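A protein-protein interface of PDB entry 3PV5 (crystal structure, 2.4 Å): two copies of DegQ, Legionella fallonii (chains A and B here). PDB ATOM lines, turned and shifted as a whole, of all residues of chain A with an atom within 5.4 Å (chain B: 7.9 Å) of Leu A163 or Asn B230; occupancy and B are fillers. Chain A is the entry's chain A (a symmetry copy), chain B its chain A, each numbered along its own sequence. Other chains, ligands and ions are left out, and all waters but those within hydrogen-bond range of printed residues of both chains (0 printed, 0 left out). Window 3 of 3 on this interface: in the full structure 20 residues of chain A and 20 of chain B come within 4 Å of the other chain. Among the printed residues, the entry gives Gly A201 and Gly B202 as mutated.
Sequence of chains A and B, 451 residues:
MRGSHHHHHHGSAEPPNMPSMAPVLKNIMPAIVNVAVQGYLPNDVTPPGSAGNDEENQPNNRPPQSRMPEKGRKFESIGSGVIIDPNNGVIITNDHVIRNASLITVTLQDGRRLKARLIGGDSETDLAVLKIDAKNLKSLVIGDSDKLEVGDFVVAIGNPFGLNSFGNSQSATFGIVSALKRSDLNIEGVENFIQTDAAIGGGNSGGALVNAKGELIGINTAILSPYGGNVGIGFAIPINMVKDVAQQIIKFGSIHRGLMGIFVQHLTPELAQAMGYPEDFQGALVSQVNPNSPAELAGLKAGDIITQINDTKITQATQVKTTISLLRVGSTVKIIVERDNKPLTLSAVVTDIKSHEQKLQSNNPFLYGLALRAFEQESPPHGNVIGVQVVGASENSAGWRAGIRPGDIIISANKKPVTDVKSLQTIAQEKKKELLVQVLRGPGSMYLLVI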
ATOM      1  N   ASN A 159     -16.108  -3.696  -9.551  1.00  0.00           N
ATOM      2  CA  ASN A 159     -16.212  -5.048  -8.996  1.00  0.00           C
ATOM      3  C   ASN A 159     -15.239  -6.008  -9.645  1.00  0.00           C
ATOM      4  O   ASN A 159     -15.019  -5.909 -10.799  1.00  0.00           O
ATOM      5  CB  ASN A 159     -17.664  -5.591  -9.063  1.00  0.00           C
ATOM      6  CG  ASN A 159     -18.569  -4.916  -8.045  1.00  0.00           C
ATOM      7  OD1 ASN A 159     -18.114  -4.577  -6.938  1.00  0.00           O
ATOM      8  ND2 ASN A 159     -19.839  -4.701  -8.400  1.00  0.00           N
ATOM      9  N   PRO A 160     -14.595  -6.881  -8.859  1.00  0.00           N
ATOM     10  CA  PRO A 160     -13.836  -8.014  -9.431  1.00  0.00           C
ATOM     11  C   PRO A 160     -14.745  -8.967 -10.217  1.00  0.00           C
ATOM     12  O   PRO A 160     -15.946  -8.832 -10.148  1.00  0.00           O
ATOM     13  CB  PRO A 160     -13.243  -8.722  -8.194  1.00  0.00           C
ATOM     14  CG  PRO A 160     -13.603  -7.893  -7.000  1.00  0.00           C
ATOM     15  CD  PRO A 160     -14.371  -6.709  -7.406  1.00  0.00           C
ATOM     16  N   PHE A 161     -14.176  -9.924 -10.946  1.00  0.00           N
ATOM     17  CA  PHE A 161     -14.994 -10.882 -11.741  1.00  0.00           C
ATOM     18  C   PHE A 161     -16.035 -11.665 -10.879  1.00  0.00           C
ATOM     19  O   PHE A 161     -17.192 -11.901 -11.299  1.00  0.00           O
ATOM     20  CB  PHE A 161     -14.104 -11.834 -12.594  1.00  0.00           C
ATOM     21  CG  PHE A 161     -14.742 -13.196 -12.900  1.00  0.00           C
ATOM     22  CD1 PHE A 161     -15.456 -13.409 -14.088  1.00  0.00           C
ATOM     23  CD2 PHE A 161     -14.624 -14.262 -11.988  1.00  0.00           C
ATOM     24  CE1 PHE A 161     -16.040 -14.658 -14.381  1.00  0.00           C
ATOM     25  CE2 PHE A 161     -15.208 -15.523 -12.263  1.00  0.00           C
ATOM     26  CZ  PHE A 161     -15.918 -15.715 -13.472  1.00  0.00           C
ATOM     27  N   GLY A 162     -15.656 -12.023  -9.664  1.00  0.00           N
ATOM     28  CA  GLY A 162     -16.618 -12.693  -8.768  1.00  0.00           C
ATOM     29  C   GLY A 162     -17.871 -11.899  -8.365  1.00  0.00           C
ATOM     30  O   GLY A 162     -18.989 -12.419  -8.438  1.00  0.00           O
ATOM     31  N   LEU A 163     -17.672 -10.624  -8.000  1.00  0.00           N
ATOM     32  CA  LEU A 163     -18.456  -9.934  -6.944  1.00  0.00           C
ATOM     33  C   LEU A 163     -19.688  -9.080  -7.328  1.00  0.00           C
ATOM     34  O   LEU A 163     -19.921  -8.779  -8.498  1.00  0.00           O
ATOM     35  CB  LEU A 163     -17.499  -9.042  -6.119  1.00  0.00           C
ATOM     36  CG  LEU A 163     -16.851  -9.569  -4.826  1.00  0.00           C
ATOM     37  CD1 LEU A 163     -17.676  -9.153  -3.603  1.00  0.00           C
ATOM     38  CD2 LEU A 163     -16.592 -11.090  -4.862  1.00  0.00           C
ATOM     39  N   ASN A 164     -20.417  -8.693  -6.265  1.00  0.00           N
ATOM     40  CA  ASN A 164     -21.700  -7.936  -6.245  1.00  0.00           C
ATOM     41  C   ASN A 164     -22.350  -7.692  -7.580  1.00  0.00           C
ATOM     42  O   ASN A 164     -22.547  -6.527  -7.997  1.00  0.00           O
ATOM     43  CB  ASN A 164     -21.562  -6.590  -5.491  1.00  0.00           C
ATOM     44  CG  ASN A 164     -22.925  -5.839  -5.324  1.00  0.00           C
ATOM     45  OD1 ASN A 164     -23.281  -4.974  -6.152  1.00  0.00           O
ATOM     46  ND2 ASN A 164     -23.675  -6.168  -4.253  1.00  0.00           N
ATOM     47  N   SER A 165     -22.712  -8.787  -8.241  1.00  0.00           N
ATOM     48  CA  SER A 165     -23.464  -8.681  -9.469  1.00  0.00           C
ATOM     49  C   SER A 165     -24.767  -7.887  -9.195  1.00  0.00           C
ATOM     50  O   SER A 165     -25.184  -7.073 -10.020  1.00  0.00           O
ATOM     51  CB  SER A 165     -23.730 -10.090 -10.020  1.00  0.00           C
ATOM     52  OG  SER A 165     -22.534 -10.872  -9.990  1.00  0.00           O
ATOM     53  N   SER A 171     -17.264  -2.097  -5.864  1.00  0.00           N
ATOM     54  CA  SER A 171     -16.188  -2.204  -4.865  1.00  0.00           C
ATOM     55  C   SER A 171     -15.090  -1.190  -5.098  1.00  0.00           C
ATOM     56  O   SER A 171     -14.684  -0.947  -6.246  1.00  0.00           O
ATOM     57  CB  SER A 171     -15.541  -3.574  -4.867  1.00  0.00           C
ATOM     58  OG  SER A 171     -16.469  -4.585  -4.489  1.00  0.00           O
ATOM     59  N   GLY A 201      -9.517  -9.290  -6.019  1.00  0.00           N
ATOM     60  CA  GLY A 201     -10.150 -10.376  -6.747  1.00  0.00           C
ATOM     61  C   GLY A 201      -9.570 -10.592  -8.145  1.00  0.00           C
ATOM     62  O   GLY A 201     -10.266 -11.069  -9.045  1.00  0.00           O
ATOM     63  N   ALA B 179     -16.736  -2.064   0.409  1.00  0.00           N
ATOM     64  CA  ALA B 179     -18.197  -2.116   0.221  1.00  0.00           C
ATOM     65  C   ALA B 179     -18.926  -2.434   1.543  1.00  0.00           C
ATOM     66  O   ALA B 179     -18.469  -3.254   2.325  1.00  0.00           O
ATOM     67  CB  ALA B 179     -18.597  -3.162  -0.842  1.00  0.00           C
ATOM     68  N   VAL B 190     -20.949 -13.429   0.422  1.00  0.00           N
ATOM     69  CA  VAL B 190     -20.111 -12.212   0.446  1.00  0.00           C
ATOM     70  C   VAL B 190     -20.974 -10.941   0.729  1.00  0.00           C
ATOM     71  O   VAL B 190     -20.557  -9.962   1.406  1.00  0.00           O
ATOM     72  CB  VAL B 190     -19.192 -12.087  -0.864  1.00  0.00           C
ATOM     73  CG1 VAL B 190     -18.681 -13.490  -1.337  1.00  0.00           C
ATOM     74  CG2 VAL B 190     -19.873 -11.366  -2.020  1.00  0.00           C
ATOM     75  N   GLU B 191     -22.202 -10.984   0.227  1.00  0.00           N
ATOM     76  CA  GLU B 191     -23.174  -9.923   0.468  1.00  0.00           C
ATOM     77  C   GLU B 191     -23.435  -9.672   1.991  1.00  0.00           C
ATOM     78  O   GLU B 191     -23.670  -8.532   2.411  1.00  0.00           O
ATOM     79  CB  GLU B 191     -24.470 -10.238  -0.322  1.00  0.00           C
ATOM     80  CG  GLU B 191     -24.470  -9.792  -1.824  1.00  0.00           C
ATOM     81  CD  GLU B 191     -23.871 -10.811  -2.857  1.00  0.00           C
ATOM     82  OE1 GLU B 191     -23.560 -11.975  -2.490  1.00  0.00           O
ATOM     83  OE2 GLU B 191     -23.734 -10.430  -4.062  1.00  0.00           O
ATOM     84  N   GLN B 195     -16.960  -5.255   3.847  1.00  0.00           N
ATOM     85  CA  GLN B 195     -15.937  -5.757   3.005  1.00  0.00           C
ATOM     86  C   GLN B 195     -14.883  -4.673   2.915  1.00  0.00           C
ATOM     87  O   GLN B 195     -15.183  -3.490   2.944  1.00  0.00           O
ATOM     88  CB  GLN B 195     -16.563  -6.162   1.681  1.00  0.00           C
ATOM     89  CG  GLN B 195     -15.597  -6.369   0.506  1.00  0.00           C
ATOM     90  CD  GLN B 195     -16.326  -6.659  -0.894  1.00  0.00           C
ATOM     91  OE1 GLN B 195     -17.303  -7.445  -0.975  1.00  0.00           O
ATOM     92  NE2 GLN B 195     -15.790  -6.029  -1.986  1.00  0.00           N
ATOM     93  N   THR B 196     -13.640  -5.120   2.831  1.00  0.00           N
ATOM     94  CA  THR B 196     -12.447  -4.341   3.000  1.00  0.00           C
ATOM     95  C   THR B 196     -11.422  -4.790   1.958  1.00  0.00           C
ATOM     96  O   THR B 196     -11.524  -5.911   1.491  1.00  0.00           O
ATOM     97  CB  THR B 196     -11.796  -4.848   4.357  1.00  0.00           C
ATOM     98  OG1 THR B 196     -10.789  -4.001   4.838  1.00  0.00           O
ATOM     99  CG2 THR B 196     -11.002  -5.993   4.080  1.00  0.00           C
ATOM    100  N   ALA B 199      -6.578  -7.486   3.893  1.00  0.00           N
ATOM    101  CA  ALA B 199      -6.503  -8.905   4.254  1.00  0.00           C
ATOM    102  C   ALA B 199      -5.175  -9.500   4.007  1.00  0.00           C
ATOM    103  O   ALA B 199      -4.498  -9.122   3.102  1.00  0.00           O
ATOM    104  CB  ALA B 199      -7.558  -9.694   3.527  1.00  0.00           C
ATOM    105  N   GLY B 202      -5.331 -14.824   3.158  1.00  0.00           N
ATOM    106  CA  GLY B 202      -6.702 -15.319   2.993  1.00  0.00           C
ATOM    107  C   GLY B 202      -7.609 -14.892   4.111  1.00  0.00           C
ATOM    108  O   GLY B 202      -8.759 -15.332   4.175  1.00  0.00           O
ATOM    109  N   GLY B 203      -7.094 -14.043   4.996  1.00  0.00           N
ATOM    110  CA  GLY B 203      -7.923 -13.325   5.957  1.00  0.00           C
ATOM    111  C   GLY B 203      -7.883 -13.876   7.375  1.00  0.00           C
ATOM    112  O   GLY B 203      -7.463 -14.982   7.608  1.00  0.00           O
ATOM    113  N   ALA B 222     -13.214 -15.231   7.872  1.00  0.00           N
ATOM    114  CA  ALA B 222     -12.487 -15.702   6.656  1.00  0.00           C
ATOM    115  C   ALA B 222     -13.169 -16.744   5.782  1.00  0.00           C
ATOM    116  O   ALA B 222     -12.887 -17.920   5.950  1.00  0.00           O
ATOM    117  CB  ALA B 222     -11.070 -16.268   7.057  1.00  0.00           C
ATOM    118  N   ILE B 223     -13.956 -16.344   4.776  1.00  0.00           N
ATOM    119  CA  ILE B 223     -14.619 -17.365   3.870  1.00  0.00           C
ATOM    120  C   ILE B 223     -13.695 -17.757   2.676  1.00  0.00           C
ATOM    121  O   ILE B 223     -12.876 -16.949   2.237  1.00  0.00           O
ATOM    122  CB  ILE B 223     -16.044 -16.920   3.432  1.00  0.00           C
ATOM    123  CG1 ILE B 223     -16.032 -16.104   2.134  1.00  0.00           C
ATOM    124  CG2 ILE B 223     -16.733 -16.125   4.589  1.00  0.00           C
ATOM    125  CD1 ILE B 223     -17.287 -15.254   1.921  1.00  0.00           C
ATOM    126  N   LEU B 224     -13.804 -18.989   2.175  1.00  0.00           N
ATOM    127  CA  LEU B 224     -12.823 -19.535   1.185  1.00  0.00           C
ATOM    128  C   LEU B 224     -13.170 -19.191  -0.286  1.00  0.00           C
ATOM    129  O   LEU B 224     -12.837 -18.104  -0.783  1.00  0.00           O
ATOM    130  CB  LEU B 224     -12.654 -21.070   1.364  1.00  0.00           C
ATOM    131  CG  LEU B 224     -11.679 -21.594   2.460  1.00  0.00           C
ATOM    132  CD1 LEU B 224     -12.140 -21.299   3.920  1.00  0.00           C
ATOM    133  CD2 LEU B 224     -11.420 -23.119   2.287  1.00  0.00           C
ATOM    134  N   ASN B 230     -11.452 -14.538  -3.818  1.00  0.00           N
ATOM    135  CA  ASN B 230     -11.580 -13.261  -3.076  1.00  0.00           C
ATOM    136  C   ASN B 230     -10.209 -12.687  -2.640  1.00  0.00           C
ATOM    137  O   ASN B 230     -10.110 -11.980  -1.649  1.00  0.00           O
ATOM    138  CB  ASN B 230     -12.486 -13.448  -1.834  1.00  0.00           C
ATOM    139  CG  ASN B 230     -13.864 -14.062  -2.195  1.00  0.00           C
ATOM    140  OD1 ASN B 230     -14.585 -13.512  -3.049  1.00  0.00           O
ATOM    141  ND2 ASN B 230     -14.215 -15.224  -1.572  1.00  0.00           N
ATOM    142  N   VAL B 231      -9.159 -13.000  -3.392  1.00  0.00           N
ATOM    143  CA  VAL B 231      -7.824 -12.571  -3.045  1.00  0.00           C
ATOM    144  C   VAL B 231      -7.751 -11.072  -2.696  1.00  0.00           C
ATOM    145  O   VAL B 231      -8.252 -10.234  -3.423  1.00  0.00           O
ATOM    146  CB  VAL B 231      -6.819 -12.950  -4.212  1.00  0.00           C
ATOM    147  CG1 VAL B 231      -5.401 -12.492  -3.895  1.00  0.00           C
ATOM    148  CG2 VAL B 231      -6.815 -14.495  -4.437  1.00  0.00           C
ATOM    149  N   GLY B 232      -7.095 -10.734  -1.592  1.00  0.00           N
ATOM    150  CA  GLY B 232      -6.950  -9.329  -1.141  1.00  0.00           C
ATOM    151  C   GLY B 232      -8.210  -8.705  -0.534  1.00  0.00           C
ATOM    152  O   GLY B 232      -8.222  -7.499  -0.225  1.00  0.00           O
ATOM    153  N   ILE B 233      -9.283  -9.484  -0.412  1.00  0.00           N
ATOM    154  CA  ILE B 233     -10.512  -8.972   0.172  1.00  0.00           C
ATOM    155  C   ILE B 233     -10.735  -9.454   1.635  1.00  0.00           C
ATOM    156  O   ILE B 233     -10.725 -10.618   1.923  1.00  0.00           O
ATOM    157  CB  ILE B 233     -11.721  -9.374  -0.649  1.00  0.00           C
ATOM    158  CG1 ILE B 233     -11.595  -8.912  -2.104  1.00  0.00           C
ATOM    159  CG2 ILE B 233     -13.017  -8.710  -0.049  1.00  0.00           C
ATOM    160  CD1 ILE B 233     -12.855  -9.417  -2.999  1.00  0.00           C
ATOM    161  N   GLY B 234     -10.977  -8.543   2.525  1.00  0.00           N
ATOM    162  CA  GLY B 234     -11.236  -8.902   3.948  1.00  0.00           C
ATOM    163  C   GLY B 234     -12.665  -8.683   4.299  1.00  0.00           C
ATOM    164  O   GLY B 234     -13.300  -7.748   3.763  1.00  0.00           O
ATOM    165  N   PHE B 235     -13.196  -9.550   5.171  1.00  0.00           N
ATOM    166  CA  PHE B 235     -14.613  -9.470   5.599  1.00  0.00           C
ATOM    167  C   PHE B 235     -14.782  -9.233   7.070  1.00  0.00           C
ATOM    168  O   PHE B 235     -14.029  -9.788   7.854  1.00  0.00           O
ATOM    169  CB  PHE B 235     -15.295 -10.783   5.255  1.00  0.00           C
ATOM    170  CG  PHE B 235     -15.234 -11.102   3.801  1.00  0.00           C
ATOM    171  CD1 PHE B 235     -16.044 -10.419   2.902  1.00  0.00           C
ATOM    172  CD2 PHE B 235     -14.342 -12.056   3.320  1.00  0.00           C
ATOM    173  CE1 PHE B 235     -15.958 -10.667   1.521  1.00  0.00           C
ATOM    174  CE2 PHE B 235     -14.266 -12.337   1.936  1.00  0.00           C
ATOM    175  CZ  PHE B 235     -15.097 -11.607   1.052  1.00  0.00           C
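NE2 of Gln B195 lies within hydrogen-bond range of OG of Ser A171 (3.0 Å). The backbone carbonyl oxygen (O) of Val B231 sits at hydrogen-bond distance from the backbone NH (N) of Gly A201, 3.0 Å away.
The backbone carbonyl oxygen (O) of Ala B179 sits at hydrogen-bond distance from the backbone NH (N) of Gln B195, 2.9 Å away. The side-chain amide nitrogen (ND2) of Asn B230 sits at hydrogen-bond distance from the backbone carbonyl oxygen (O) of Leu B224, at 3.3 Å. The side-chain amide nitrogen (ND2) of Asn A159 sits at hydrogen-bond distance from the backbone carbonyl oxygen (O) of Asn A164. OD1 of Asn A159 lies within hydrogen-bond range of N of Ser A171 (2.8 Å).
Leu A163 touches Val B190 (CD1 to CG2, 3.5 Å). Leu A163 touches Gln B195 (CD1 to OE1, 3.2 Å). Leu A163 touches Asn B230 (CD2 to OD1, 3.6 Å). Glu B191 touches Asn A164 (OE2 to CA, 3.9 Å).
Asn B230 touches just one residue of chain A: Leu A163 (3.6 Å). No residue of chain B comes within 4 Å of Gly A162. Of the printed residues of chain B, Ser A171 touches Gln B195 (3.0 Å). Of the printed residues of chain B, Gly A201 touches Val B231 (3.0 Å). Of the printed residues of chain A, Gln B195 touches Leu A163 (3.2 Å) and Ser A171 (3.0 Å). The nearest residue of chain A that does not touch Asn B230 is Gly A201 (4.7 Å). The nearest printed residue of chain A that does not touch Val B231 is Pro A160 (6.8 Å).
Along chain A the printed residues that touch a printed residue of chain B span positions 163 to 201. Among the printed residues, 6 pairs touch across the chains.
No position is printed for both chains.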
